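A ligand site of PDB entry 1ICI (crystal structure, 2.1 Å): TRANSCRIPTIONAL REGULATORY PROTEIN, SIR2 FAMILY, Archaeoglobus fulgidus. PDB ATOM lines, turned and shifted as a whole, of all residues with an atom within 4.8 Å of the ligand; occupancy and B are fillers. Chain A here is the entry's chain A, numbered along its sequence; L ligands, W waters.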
ATOM      1  N   GLY A  31      24.999  -3.406 -28.345  1.00  0.00           N
ATOM      2  CA  GLY A  31      24.966  -2.155 -27.623  1.00  0.00           C
ATOM      3  C   GLY A  31      26.113  -1.294 -28.120  1.00  0.00           C
ATOM      4  O   GLY A  31      26.885  -1.727 -29.000  1.00  0.00           O
ATOM      5  N   ALA A  32      26.266  -0.099 -27.563  1.00  0.00           N
ATOM      6  CA  ALA A  32      27.299   0.842 -27.997  1.00  0.00           C
ATOM      7  C   ALA A  32      28.728   0.313 -28.020  1.00  0.00           C
ATOM      8  O   ALA A  32      29.572   0.823 -28.746  1.00  0.00           O
ATOM      9  CB  ALA A  32      27.232   2.136 -27.147  1.00  0.00           C
ATOM     10  N   GLY A  33      28.995  -0.735 -27.239  1.00  0.00           N
ATOM     11  CA  GLY A  33      30.345  -1.267 -27.184  1.00  0.00           C
ATOM     12  C   GLY A  33      30.824  -1.854 -28.489  1.00  0.00           C
ATOM     13  O   GLY A  33      32.025  -1.932 -28.763  1.00  0.00           O
ATOM     14  N   VAL A  34      29.880  -2.254 -29.321  1.00  0.00           N
ATOM     15  CA  VAL A  34      30.155  -2.859 -30.616  1.00  0.00           C
ATOM     16  C   VAL A  34      30.750  -1.846 -31.636  1.00  0.00           C
ATOM     17  O   VAL A  34      31.348  -2.229 -32.642  1.00  0.00           O
ATOM     18  CB  VAL A  34      28.831  -3.515 -31.112  1.00  0.00           C
ATOM     19  CG1 VAL A  34      28.615  -3.274 -32.581  1.00  0.00           C
ATOM     20  CG2 VAL A  34      28.842  -5.034 -30.747  1.00  0.00           C
ATOM     21  N   ALA A  36      32.574   0.891 -30.323  1.00  0.00           N
ATOM     22  CA  ALA A  36      33.697   1.547 -29.662  1.00  0.00           C
ATOM     23  C   ALA A  36      34.979   1.422 -30.499  1.00  0.00           C
ATOM     24  O   ALA A  36      35.792   2.336 -30.543  1.00  0.00           O
ATOM     25  CB  ALA A  36      33.912   0.960 -28.271  1.00  0.00           C
ATOM     26  N   GLU A  37      35.136   0.291 -31.190  1.00  0.00           N
ATOM     27  CA  GLU A  37      36.343   0.097 -31.973  1.00  0.00           C
ATOM     28  C   GLU A  37      36.287   0.753 -33.350  1.00  0.00           C
ATOM     29  O   GLU A  37      37.156   0.539 -34.186  1.00  0.00           O
ATOM     30  CB  GLU A  37      36.654  -1.399 -32.087  1.00  0.00           C
ATOM     31  CG  GLU A  37      36.984  -2.026 -30.716  1.00  0.00           C
ATOM     32  CD  GLU A  37      36.953  -3.554 -30.736  1.00  0.00           C
ATOM     33  OE1 GLU A  37      37.864  -4.174 -31.324  1.00  0.00           O
ATOM     34  OE2 GLU A  37      35.994  -4.136 -30.185  1.00  0.00           O
ATOM     35  N   THR A  42      31.859   4.750 -25.906  1.00  0.00           N
ATOM     36  CA  THR A  42      30.650   4.603 -25.126  1.00  0.00           C
ATOM     37  C   THR A  42      30.758   5.893 -24.304  1.00  0.00           C
ATOM     38  O   THR A  42      31.871   6.386 -24.107  1.00  0.00           O
ATOM     39  CB  THR A  42      30.760   3.358 -24.244  1.00  0.00           C
ATOM     40  OG1 THR A  42      31.975   3.421 -23.483  1.00  0.00           O
ATOM     41  CG2 THR A  42      30.792   2.104 -25.106  1.00  0.00           C
ATOM     42  N   PHE A  43      29.647   6.456 -23.837  1.00  0.00           N
ATOM     43  CA  PHE A  43      29.703   7.719 -23.090  1.00  0.00           C
ATOM     44  C   PHE A  43      30.179   7.647 -21.647  1.00  0.00           C
ATOM     45  O   PHE A  43      30.632   8.651 -21.087  1.00  0.00           O
ATOM     46  CB  PHE A  43      28.353   8.443 -23.136  1.00  0.00           C
ATOM     47  CG  PHE A  43      27.998   8.949 -24.501  1.00  0.00           C
ATOM     48  CD1 PHE A  43      27.092   8.247 -25.308  1.00  0.00           C
ATOM     49  CD2 PHE A  43      28.617  10.086 -25.009  1.00  0.00           C
ATOM     50  CE1 PHE A  43      26.819   8.676 -26.606  1.00  0.00           C
ATOM     51  CE2 PHE A  43      28.347  10.521 -26.319  1.00  0.00           C
ATOM     52  CZ  PHE A  43      27.446   9.812 -27.120  1.00  0.00           C
ATOM     53  N   ARG A  44      30.067   6.468 -21.040  1.00  0.00           N
ATOM     54  CA  ARG A  44      30.499   6.277 -19.660  1.00  0.00           C
ATOM     55  C   ARG A  44      30.032   7.395 -18.746  1.00  0.00           C
ATOM     56  O   ARG A  44      30.794   7.842 -17.882  1.00  0.00           O
ATOM     57  CB  ARG A  44      32.022   6.177 -19.591  1.00  0.00           C
ATOM     58  CG  ARG A  44      32.598   4.976 -20.329  1.00  0.00           C
ATOM     59  CD  ARG A  44      34.056   5.221 -20.641  1.00  0.00           C
ATOM     60  NE  ARG A  44      34.540   4.275 -21.634  1.00  0.00           N
ATOM     61  CZ  ARG A  44      35.643   4.445 -22.353  1.00  0.00           C
ATOM     62  NH1 ARG A  44      36.386   5.535 -22.195  1.00  0.00           N
ATOM     63  NH2 ARG A  44      36.010   3.525 -23.238  1.00  0.00           N
ATOM     64  N   GLY A  45      28.801   7.864 -18.935  1.00  0.00           N
ATOM     65  CA  GLY A  45      28.269   8.898 -18.078  1.00  0.00           C
ATOM     66  C   GLY A  45      28.500  10.369 -18.422  1.00  0.00           C
ATOM     67  O   GLY A  45      27.930  11.237 -17.770  1.00  0.00           O
ATOM     68  N   PRO A  55      24.653  11.492 -20.565  1.00  0.00           N
ATOM     69  CA  PRO A  55      23.954  11.483 -21.864  1.00  0.00           C
ATOM     70  C   PRO A  55      22.428  11.675 -21.742  1.00  0.00           C
ATOM     71  O   PRO A  55      21.823  12.446 -22.504  1.00  0.00           O
ATOM     72  CB  PRO A  55      24.323  10.123 -22.453  1.00  0.00           C
ATOM     73  CG  PRO A  55      25.651   9.813 -21.791  1.00  0.00           C
ATOM     74  CD  PRO A  55      25.436  10.266 -20.374  1.00  0.00           C
ATOM     75  N   GLU A  56      21.832  10.977 -20.781  1.00  0.00           N
ATOM     76  CA  GLU A  56      20.385  11.038 -20.546  1.00  0.00           C
ATOM     77  C   GLU A  56      19.805  12.448 -20.341  1.00  0.00           C
ATOM     78  O   GLU A  56      18.607  12.651 -20.496  1.00  0.00           O
ATOM     79  CB  GLU A  56      20.038  10.181 -19.336  1.00  0.00           C
ATOM     80  CG  GLU A  56      20.667  10.683 -18.062  1.00  0.00           C
ATOM     81  CD  GLU A  56      21.432   9.604 -17.315  1.00  0.00           C
ATOM     82  OE1 GLU A  56      22.325   8.981 -17.925  1.00  0.00           O
ATOM     83  OE2 GLU A  56      21.115   9.391 -16.128  1.00  0.00           O
ATOM     84  N   GLN A 109      20.750  -1.502 -30.328  1.00  0.00           N
ATOM     85  CA  GLN A 109      20.303  -0.379 -29.544  1.00  0.00           C
ATOM     86  C   GLN A 109      21.060   0.836 -30.095  1.00  0.00           C
ATOM     87  O   GLN A 109      20.725   1.976 -29.794  1.00  0.00           O
ATOM     88  CB  GLN A 109      20.668  -0.586 -28.057  1.00  0.00           C
ATOM     89  CG  GLN A 109      20.161  -1.910 -27.442  1.00  0.00           C
ATOM     90  CD  GLN A 109      20.704  -2.167 -26.038  1.00  0.00           C
ATOM     91  OE1 GLN A 109      20.274  -1.547 -25.060  1.00  0.00           O
ATOM     92  NE2 GLN A 109      21.661  -3.082 -25.933  1.00  0.00           N
ATOM     93  N   ASN A 110      22.080   0.571 -30.907  1.00  0.00           N
ATOM     94  CA  ASN A 110      22.890   1.646 -31.452  1.00  0.00           C
ATOM     95  C   ASN A 110      22.137   2.523 -32.452  1.00  0.00           C
ATOM     96  O   ASN A 110      21.231   2.048 -33.159  1.00  0.00           O
ATOM     97  CB  ASN A 110      24.161   1.102 -32.115  1.00  0.00           C
ATOM     98  CG  ASN A 110      25.054   0.363 -31.128  1.00  0.00           C
ATOM     99  OD1 ASN A 110      24.901   0.476 -29.917  1.00  0.00           O
ATOM    100  ND2 ASN A 110      26.023  -0.393 -31.659  1.00  0.00           N
ATOM    101  N   HIS A 127      16.254   1.642 -30.963  1.00  0.00           N
ATOM    102  CA  HIS A 127      16.231   3.010 -30.495  1.00  0.00           C
ATOM    103  C   HIS A 127      16.396   4.055 -31.585  1.00  0.00           C
ATOM    104  O   HIS A 127      16.927   5.131 -31.335  1.00  0.00           O
ATOM    105  CB  HIS A 127      17.327   3.210 -29.447  1.00  0.00           C
ATOM    106  CG  HIS A 127      17.239   2.256 -28.301  1.00  0.00           C
ATOM    107  ND1 HIS A 127      18.308   2.001 -27.467  1.00  0.00           N
ATOM    108  CD2 HIS A 127      16.220   1.487 -27.858  1.00  0.00           C
ATOM    109  CE1 HIS A 127      17.945   1.115 -26.549  1.00  0.00           C
ATOM    110  NE2 HIS A 127      16.680   0.786 -26.762  1.00  0.00           N
ATOM    111  N   GLY A 196      28.524  -6.014 -26.499  1.00  0.00           N
ATOM    112  CA  GLY A 196      28.692  -4.591 -26.316  1.00  0.00           C
ATOM    113  C   GLY A 196      27.553  -3.837 -25.646  1.00  0.00           C
ATOM    114  O   GLY A 196      27.363  -2.666 -25.944  1.00  0.00           O
ATOM    115  N   THR A 197      26.796  -4.496 -24.766  1.00  0.00           N
ATOM    116  CA  THR A 197      25.738  -3.772 -24.061  1.00  0.00           C
ATOM    117  C   THR A 197      25.799  -3.934 -22.530  1.00  0.00           C
ATOM    118  O   THR A 197      26.074  -5.030 -22.013  1.00  0.00           O
ATOM    119  CB  THR A 197      24.307  -4.154 -24.555  1.00  0.00           C
ATOM    120  OG1 THR A 197      23.329  -3.551 -23.692  1.00  0.00           O
ATOM    121  CG2 THR A 197      24.110  -5.672 -24.583  1.00  0.00           C
ATOM    122  N   SER A 198      25.550  -2.839 -21.821  1.00  0.00           N
ATOM    123  CA  SER A 198      25.563  -2.860 -20.367  1.00  0.00           C
ATOM    124  C   SER A 198      24.398  -3.634 -19.740  1.00  0.00           C
ATOM    125  O   SER A 198      24.377  -3.852 -18.547  1.00  0.00           O
ATOM    126  CB  SER A 198      25.609  -1.420 -19.806  1.00  0.00           C
ATOM    127  OG  SER A 198      24.571  -0.609 -20.337  1.00  0.00           O
ATOM    128  N   ALA A 199      23.431  -4.049 -20.569  1.00  0.00           N
ATOM    129  CA  ALA A 199      22.293  -4.843 -20.124  1.00  0.00           C
ATOM    130  C   ALA A 199      21.481  -4.262 -18.961  1.00  0.00           C
ATOM    131  O   ALA A 199      21.091  -4.979 -18.036  1.00  0.00           O
ATOM    132  CB  ALA A 199      22.740  -6.287 -19.778  1.00  0.00           C
ATOM    133  N   VAL A 201      19.516  -0.877 -19.720  1.00  0.00           N
ATOM    134  CA  VAL A 201      18.422  -0.146 -20.344  1.00  0.00           C
ATOM    135  C   VAL A 201      17.362  -1.096 -20.890  1.00  0.00           C
ATOM    136  O   VAL A 201      17.672  -2.015 -21.641  1.00  0.00           O
ATOM    137  CB  VAL A 201      18.927   0.772 -21.464  1.00  0.00           C
ATOM    138  CG1 VAL A 201      17.747   1.309 -22.286  1.00  0.00           C
ATOM    139  CG2 VAL A 201      19.706   1.924 -20.854  1.00  0.00           C
ATOM    140  N   ILE A 221      29.123 -11.203 -24.951  1.00  0.00           N
ATOM    141  CA  ILE A 221      30.478 -10.762 -25.268  1.00  0.00           C
ATOM    142  C   ILE A 221      30.628  -9.368 -24.691  1.00  0.00           C
ATOM    143  O   ILE A 221      30.040  -8.416 -25.212  1.00  0.00           O
ATOM    144  CB  ILE A 221      30.719 -10.712 -26.796  1.00  0.00           C
ATOM    145  CG1 ILE A 221      30.570 -12.101 -27.403  1.00  0.00           C
ATOM    146  CG2 ILE A 221      32.087 -10.119 -27.073  1.00  0.00           C
ATOM    147  CD1 ILE A 221      30.615 -12.161 -28.909  1.00  0.00           C
ATOM    148  N   ASN A 222      31.425  -9.231 -23.621  1.00  0.00           N
ATOM    149  CA  ASN A 222      31.597  -7.937 -22.969  1.00  0.00           C
ATOM    150  C   ASN A 222      32.855  -7.966 -22.123  1.00  0.00           C
ATOM    151  O   ASN A 222      33.135  -8.952 -21.453  1.00  0.00           O
ATOM    152  CB  ASN A 222      30.398  -7.640 -22.043  1.00  0.00           C
ATOM    153  CG  ASN A 222      30.275  -6.149 -21.679  1.00  0.00           C
ATOM    154  OD1 ASN A 222      31.226  -5.525 -21.185  1.00  0.00           O
ATOM    155  ND2 ASN A 222      29.105  -5.577 -21.941  1.00  0.00           N
ATOM    156  N   PRO A 223      33.641  -6.883 -22.160  1.00  0.00           N
ATOM    157  CA  PRO A 223      34.857  -6.866 -21.349  1.00  0.00           C
ATOM    158  C   PRO A 223      34.466  -6.727 -19.879  1.00  0.00           C
ATOM    159  O   PRO A 223      35.300  -6.901 -18.998  1.00  0.00           O
ATOM    160  CB  PRO A 223      35.616  -5.650 -21.882  1.00  0.00           C
ATOM    161  CG  PRO A 223      34.541  -4.771 -22.444  1.00  0.00           C
ATOM    162  CD  PRO A 223      33.621  -5.762 -23.116  1.00  0.00           C
ATOM    163  N   ASP A 224      33.185  -6.454 -19.630  1.00  0.00           N
ATOM    164  CA  ASP A 224      32.648  -6.319 -18.267  1.00  0.00           C
ATOM    165  C   ASP A 224      31.557  -7.346 -18.019  1.00  0.00           C
ATOM    166  O   ASP A 224      30.950  -7.873 -18.961  1.00  0.00           O
ATOM    167  CB  ASP A 224      31.974  -4.947 -18.062  1.00  0.00           C
ATOM    168  CG  ASP A 224      32.954  -3.821 -17.784  1.00  0.00           C
ATOM    169  OD1 ASP A 224      34.155  -4.068 -17.562  1.00  0.00           O
ATOM    170  OD2 ASP A 224      32.490  -2.650 -17.787  1.00  0.00           O
ATOM    171  N   THR A 226      27.790  -8.081 -16.520  1.00  0.00           N
ATOM    172  CA  THR A 226      26.617  -7.223 -16.459  1.00  0.00           C
ATOM    173  C   THR A 226      25.477  -7.957 -15.775  1.00  0.00           C
ATOM    174  O   THR A 226      25.626  -9.099 -15.341  1.00  0.00           O
ATOM    175  CB  THR A 226      26.152  -6.809 -17.871  1.00  0.00           C
ATOM    176  OG1 THR A 226      25.631  -7.958 -18.535  1.00  0.00           O
ATOM    177  CG2 THR A 226      27.308  -6.254 -18.683  1.00  0.00           C
ATOM    178  N   GLY A 238      36.067  -9.877 -23.500  1.00  0.00           N
ATOM    179  CA  GLY A 238      36.969  -9.366 -24.511  1.00  0.00           C
ATOM    180  C   GLY A 238      36.244  -8.349 -25.361  1.00  0.00           C
ATOM    181  O   GLY A 238      35.031  -8.175 -25.228  1.00  0.00           O
ATOM    182  N   LYS A 239      36.980  -7.669 -26.236  1.00  0.00           N
ATOM    183  CA  LYS A 239      36.391  -6.680 -27.126  1.00  0.00           C
ATOM    184  C   LYS A 239      35.624  -7.408 -28.230  1.00  0.00           C
ATOM    185  O   LYS A 239      36.065  -8.457 -28.687  1.00  0.00           O
ATOM    186  CB  LYS A 239      37.497  -5.822 -27.747  1.00  0.00           C
ATOM    187  CG  LYS A 239      38.098  -4.792 -26.803  1.00  0.00           C
ATOM    188  CD  LYS A 239      39.129  -3.944 -27.526  1.00  0.00           C
ATOM    189  CE  LYS A 239      39.484  -2.717 -26.706  1.00  0.00           C
ATOM    190  NZ  LYS A 239      39.971  -3.100 -25.345  1.00  0.00           N
ATOM    191  N   ALA A 240      34.492  -6.853 -28.645  1.00  0.00           N
ATOM    192  CA  ALA A 240      33.684  -7.500 -29.692  1.00  0.00           C
ATOM    193  C   ALA A 240      34.437  -7.688 -31.001  1.00  0.00           C
ATOM    194  O   ALA A 240      34.189  -8.656 -31.724  1.00  0.00           O
ATOM    195  CB  ALA A 240      32.414  -6.697 -29.955  1.00  0.00           C
HETATM  196  P1  LIG L   1      26.513   1.370 -22.638  1.00  0.00           P
HETATM  197  O1  LIG L   1      27.392   2.553 -22.709  1.00  0.00           O
HETATM  198  O2  LIG L   1      25.578   1.477 -21.490  1.00  0.00           O
HETATM  199  O3  LIG L   1      27.377   0.029 -22.486  1.00  0.00           O
HETATM  200  C1  LIG L   1      28.391  -0.319 -23.471  1.00  0.00           C
HETATM  201  C2  LIG L   1      28.875  -1.683 -23.100  1.00  0.00           C
HETATM  202  O4  LIG L   1      29.895  -2.189 -24.010  1.00  0.00           O
HETATM  203  C3  LIG L   1      29.452  -1.804 -21.692  1.00  0.00           C
HETATM  204  O5  LIG L   1      28.869  -2.959 -21.065  1.00  0.00           O
HETATM  205  C4  LIG L   1      30.981  -1.854 -22.000  1.00  0.00           C
HETATM  206  O6  LIG L   1      31.710  -2.573 -20.975  1.00  0.00           O
HETATM  207  C5  LIG L   1      31.001  -2.615 -23.294  1.00  0.00           C
HETATM  208  N1  LIG L   1      32.151  -2.390 -24.144  1.00  0.00           N
HETATM  209  C6  LIG L   1      33.078  -1.387 -24.183  1.00  0.00           C
HETATM  210  N2  LIG L   1      33.998  -1.554 -25.162  1.00  0.00           N
HETATM  211  C7  LIG L   1      33.623  -2.736 -25.762  1.00  0.00           C
HETATM  212  C8  LIG L   1      34.161  -3.469 -26.870  1.00  0.00           C
HETATM  213  N3  LIG L   1      35.240  -3.069 -27.534  1.00  0.00           N
HETATM  214  N4  LIG L   1      33.526  -4.635 -27.236  1.00  0.00           N
HETATM  215  C9  LIG L   1      32.406  -5.026 -26.528  1.00  0.00           C
HETATM  216  N5  LIG L   1      31.846  -4.399 -25.503  1.00  0.00           N
HETATM  217  C10 LIG L   1      32.496  -3.264 -25.164  1.00  0.00           C
HETATM  218  O7  LIG L   1      25.733   1.200 -23.963  1.00  0.00           O
HETATM  219  P2  LIG L   1      24.377   0.350 -24.289  1.00  0.00           P
HETATM  220  O8  LIG L   1      24.171  -0.794 -23.379  1.00  0.00           O
HETATM  221  O9  LIG L   1      24.380  -0.136 -25.690  1.00  0.00           O
HETATM  222  O10 LIG L   1      23.320   1.476 -24.197  1.00  0.00           O
HETATM  223  C11 LIG L   1      21.905   1.139 -24.092  1.00  0.00           C
HETATM  224  C12 LIG L   1      21.172   2.439 -24.259  1.00  0.00           C
HETATM  225  O11 LIG L   1      21.447   3.348 -23.198  1.00  0.00           O
HETATM  226  C13 LIG L   1      21.630   3.210 -25.520  1.00  0.00           C
HETATM  227  O12 LIG L   1      21.207   2.686 -26.800  1.00  0.00           O
HETATM  228  C14 LIG L   1      21.184   4.662 -25.192  1.00  0.00           C
HETATM  229  O13 LIG L   1      19.911   4.891 -25.819  1.00  0.00           O
HETATM  230  C15 LIG L   1      21.081   4.643 -23.674  1.00  0.00           C
HETATM  231  N6  LIG L   1      21.908   5.635 -22.940  1.00  0.00           N
HETATM  232  C16 LIG L   1      23.222   5.421 -23.185  1.00  0.00           C
HETATM  233  C17 LIG L   1      24.053   6.038 -22.447  1.00  0.00           C
HETATM  234  C18 LIG L   1      25.496   5.953 -22.517  1.00  0.00           C
HETATM  235  O14 LIG L   1      26.074   6.641 -21.677  1.00  0.00           O
HETATM  236  N7  LIG L   1      26.145   5.166 -23.433  1.00  0.00           N
HETATM  237  C19 LIG L   1      23.675   6.989 -21.331  1.00  0.00           C
HETATM  238  C20 LIG L   1      22.266   7.143 -21.194  1.00  0.00           C
HETATM  239  C21 LIG L   1      21.313   6.499 -21.965  1.00  0.00           C
HETATM  240  O   HOH W   1      23.540   1.446 -27.782  1.00  0.00           O
HETATM  241  O   HOH W   2      37.283  -0.605 -27.136  1.00  0.00           O
HETATM  242  O   HOH W   3      24.439   7.009 -25.392  1.00  0.00           O
HETATM  243  O   HOH W   4      23.901   4.276 -28.016  1.00  0.00           O
HETATM  244  O   HOH W   5      23.286   3.339 -20.944  1.00  0.00           O
HETATM  245  O   HOH W   6      35.466   0.720 -25.100  1.00  0.00           O
HETATM  246  O   HOH W   7      32.613   1.153 -22.162  1.00  0.00           O
HETATM  247  O   HOH W   8      28.988   3.945 -21.086  1.00  0.00           O
HETATM  248  O   HOH W   9      26.395   1.730 -18.855  1.00  0.00           O
HETATM  249  O   HOH W  10      20.973   9.168 -23.049  1.00  0.00           O
HETATM  250  O   HOH W  11      29.483  -2.425 -18.478  1.00  0.00           O
HETATM  251  O   HOH W  12      21.987  -0.977 -21.064  1.00  0.00           O
HETATM  252  O   HOH W  13      17.536   4.530 -24.315  1.00  0.00           O
HETATM  253  O   HOH W  14      26.026   5.221 -26.695  1.00  0.00           O
HETATM  254  O   HOH W  15      34.405  -1.918 -20.636  1.00  0.00           O
HETATM  255  O   HOH W  16      20.362   4.879 -28.480  1.00  0.00           O
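O12 of the ligand sits at hydrogen-bond distance from ND1 of His 127, 3.1 Å away. OG1 of Thr 197 is in hydrogen-bond range of O8 of the ligand (2.9 Å). OG of Ser 198 is in hydrogen-bond range of O2 of the ligand (2.6 Å). OE2 of Glu 37 lies within hydrogen-bond range of N3 of the ligand. A nitrogen (N4) of the ligand is in hydrogen-bond range of the backbone NH of Ala 240 (2.8 Å). O5 of the ligand sits at hydrogen-bond distance from ND2 of Asn 222 (2.8 Å). OD2 of Asp 224 lies within hydrogen-bond range of O6 of the ligand (3.3 Å). The backbone NH of Ala 32 is in hydrogen-bond range of an oxygen (O9) of the ligand (2.7 Å). The backbone NH (N) of Ser 198 sits at hydrogen-bond distance from an oxygen (O8) of the ligand, at 2.9 Å. O of Gln 109 is in hydrogen-bond range of O12 of the ligand (3.1 Å).
The backbone NH (N) of Ala 32 is in hydrogen-bond range of the backbone carbonyl oxygen (O) of Gly 196 (3.2 Å). N of Gly 196 lies within hydrogen-bond range of O of Ile 221. A ring nitrogen (ND1) of His 127 sits at hydrogen-bond distance from the backbone carbonyl oxygen (O) of Gln 109. O of Gly 196 sits at hydrogen-bond distance from N of Gly 33 (2.8 Å). The side-chain amide oxygen (OD1) of Asn 222 sits at hydrogen-bond distance from the backbone NH (N) of Asp 224, 2.7 Å away. The side-chain hydroxyl (OG1) of Thr 197 sits close to the backbone NH (N) of Ala 199 (3.2 Å). The side-chain hydroxyl (OG1) of Thr 42 sits at hydrogen-bond distance from the guanidinium group (NE) of Arg 44, at 3.3 Å. The side-chain amide nitrogen of Gln 109 lies within hydrogen-bond range of the side-chain hydroxyl of Thr 197 (2.8 Å).
The backbone carbonyl oxygen (O) of Gly 33 sits close to a nitrogen (N4) of the ligand, at 3.4 Å. O of Gly 196 lies close to O4 of the ligand (3.2 Å). Gly 31 touches the ligand (CA to O9, 2.9 Å). Ala 36 touches the ligand (CB to N2, 3.999 Å). CG2 of Thr 42 touches C1 of the ligand (3.8 Å). Phe 43 touches the ligand (CB to O14, 3.3 Å). CG of Pro 55 touches O14 of the ligand, at 3.2 Å. Glu 56 touches the ligand. Val 201 touches the ligand. CD of Pro 223 touches N5 of the ligand, at 3.3 Å. Lys 239 touches the ligand. Hydrophobic or aromatic side chains that line the ligand: Ala 32, Ala 36, Phe 43, Pro 55, His 127, Val 201, Pro 223 and Ala 240. The nearest printed residue that does not touch the ligand is Arg 44 (4.05 Å).
Water W8 lies within hydrogen-bond range of an oxygen (O1) of the ligand (2.7 Å) and the backbone NH of Arg 44 (2.7 Å). Water W16 lies within hydrogen-bond range of an oxygen (O13) of the ligand (2.7 Å) and the backbone carbonyl oxygen (O) of Gln 109 (3.2 Å). Water W6 bridges a nitrogen (N2) of the ligand (2.7 Å) and the guanidinium group (NH2) of Arg 44 (3.4 Å). Water W1 lies within hydrogen-bond range of OD1 of Asn 110 (2.7 Å), O9 of the ligand (2.8 Å) and N of Ala 32 (3.1 Å). Water W9 bridges O2 of the ligand (2.8 Å) and OG of Ser 198 (3.3 Å). Water W12 lies within hydrogen-bond range of the side-chain hydroxyl (OG) of Ser 198 (2.7 Å), the backbone NH (N) of Val 201 (2.8 Å), an oxygen (O8) of the ligand (3.2 Å) and the backbone NH (N) of Ala 199 (3.4 Å).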
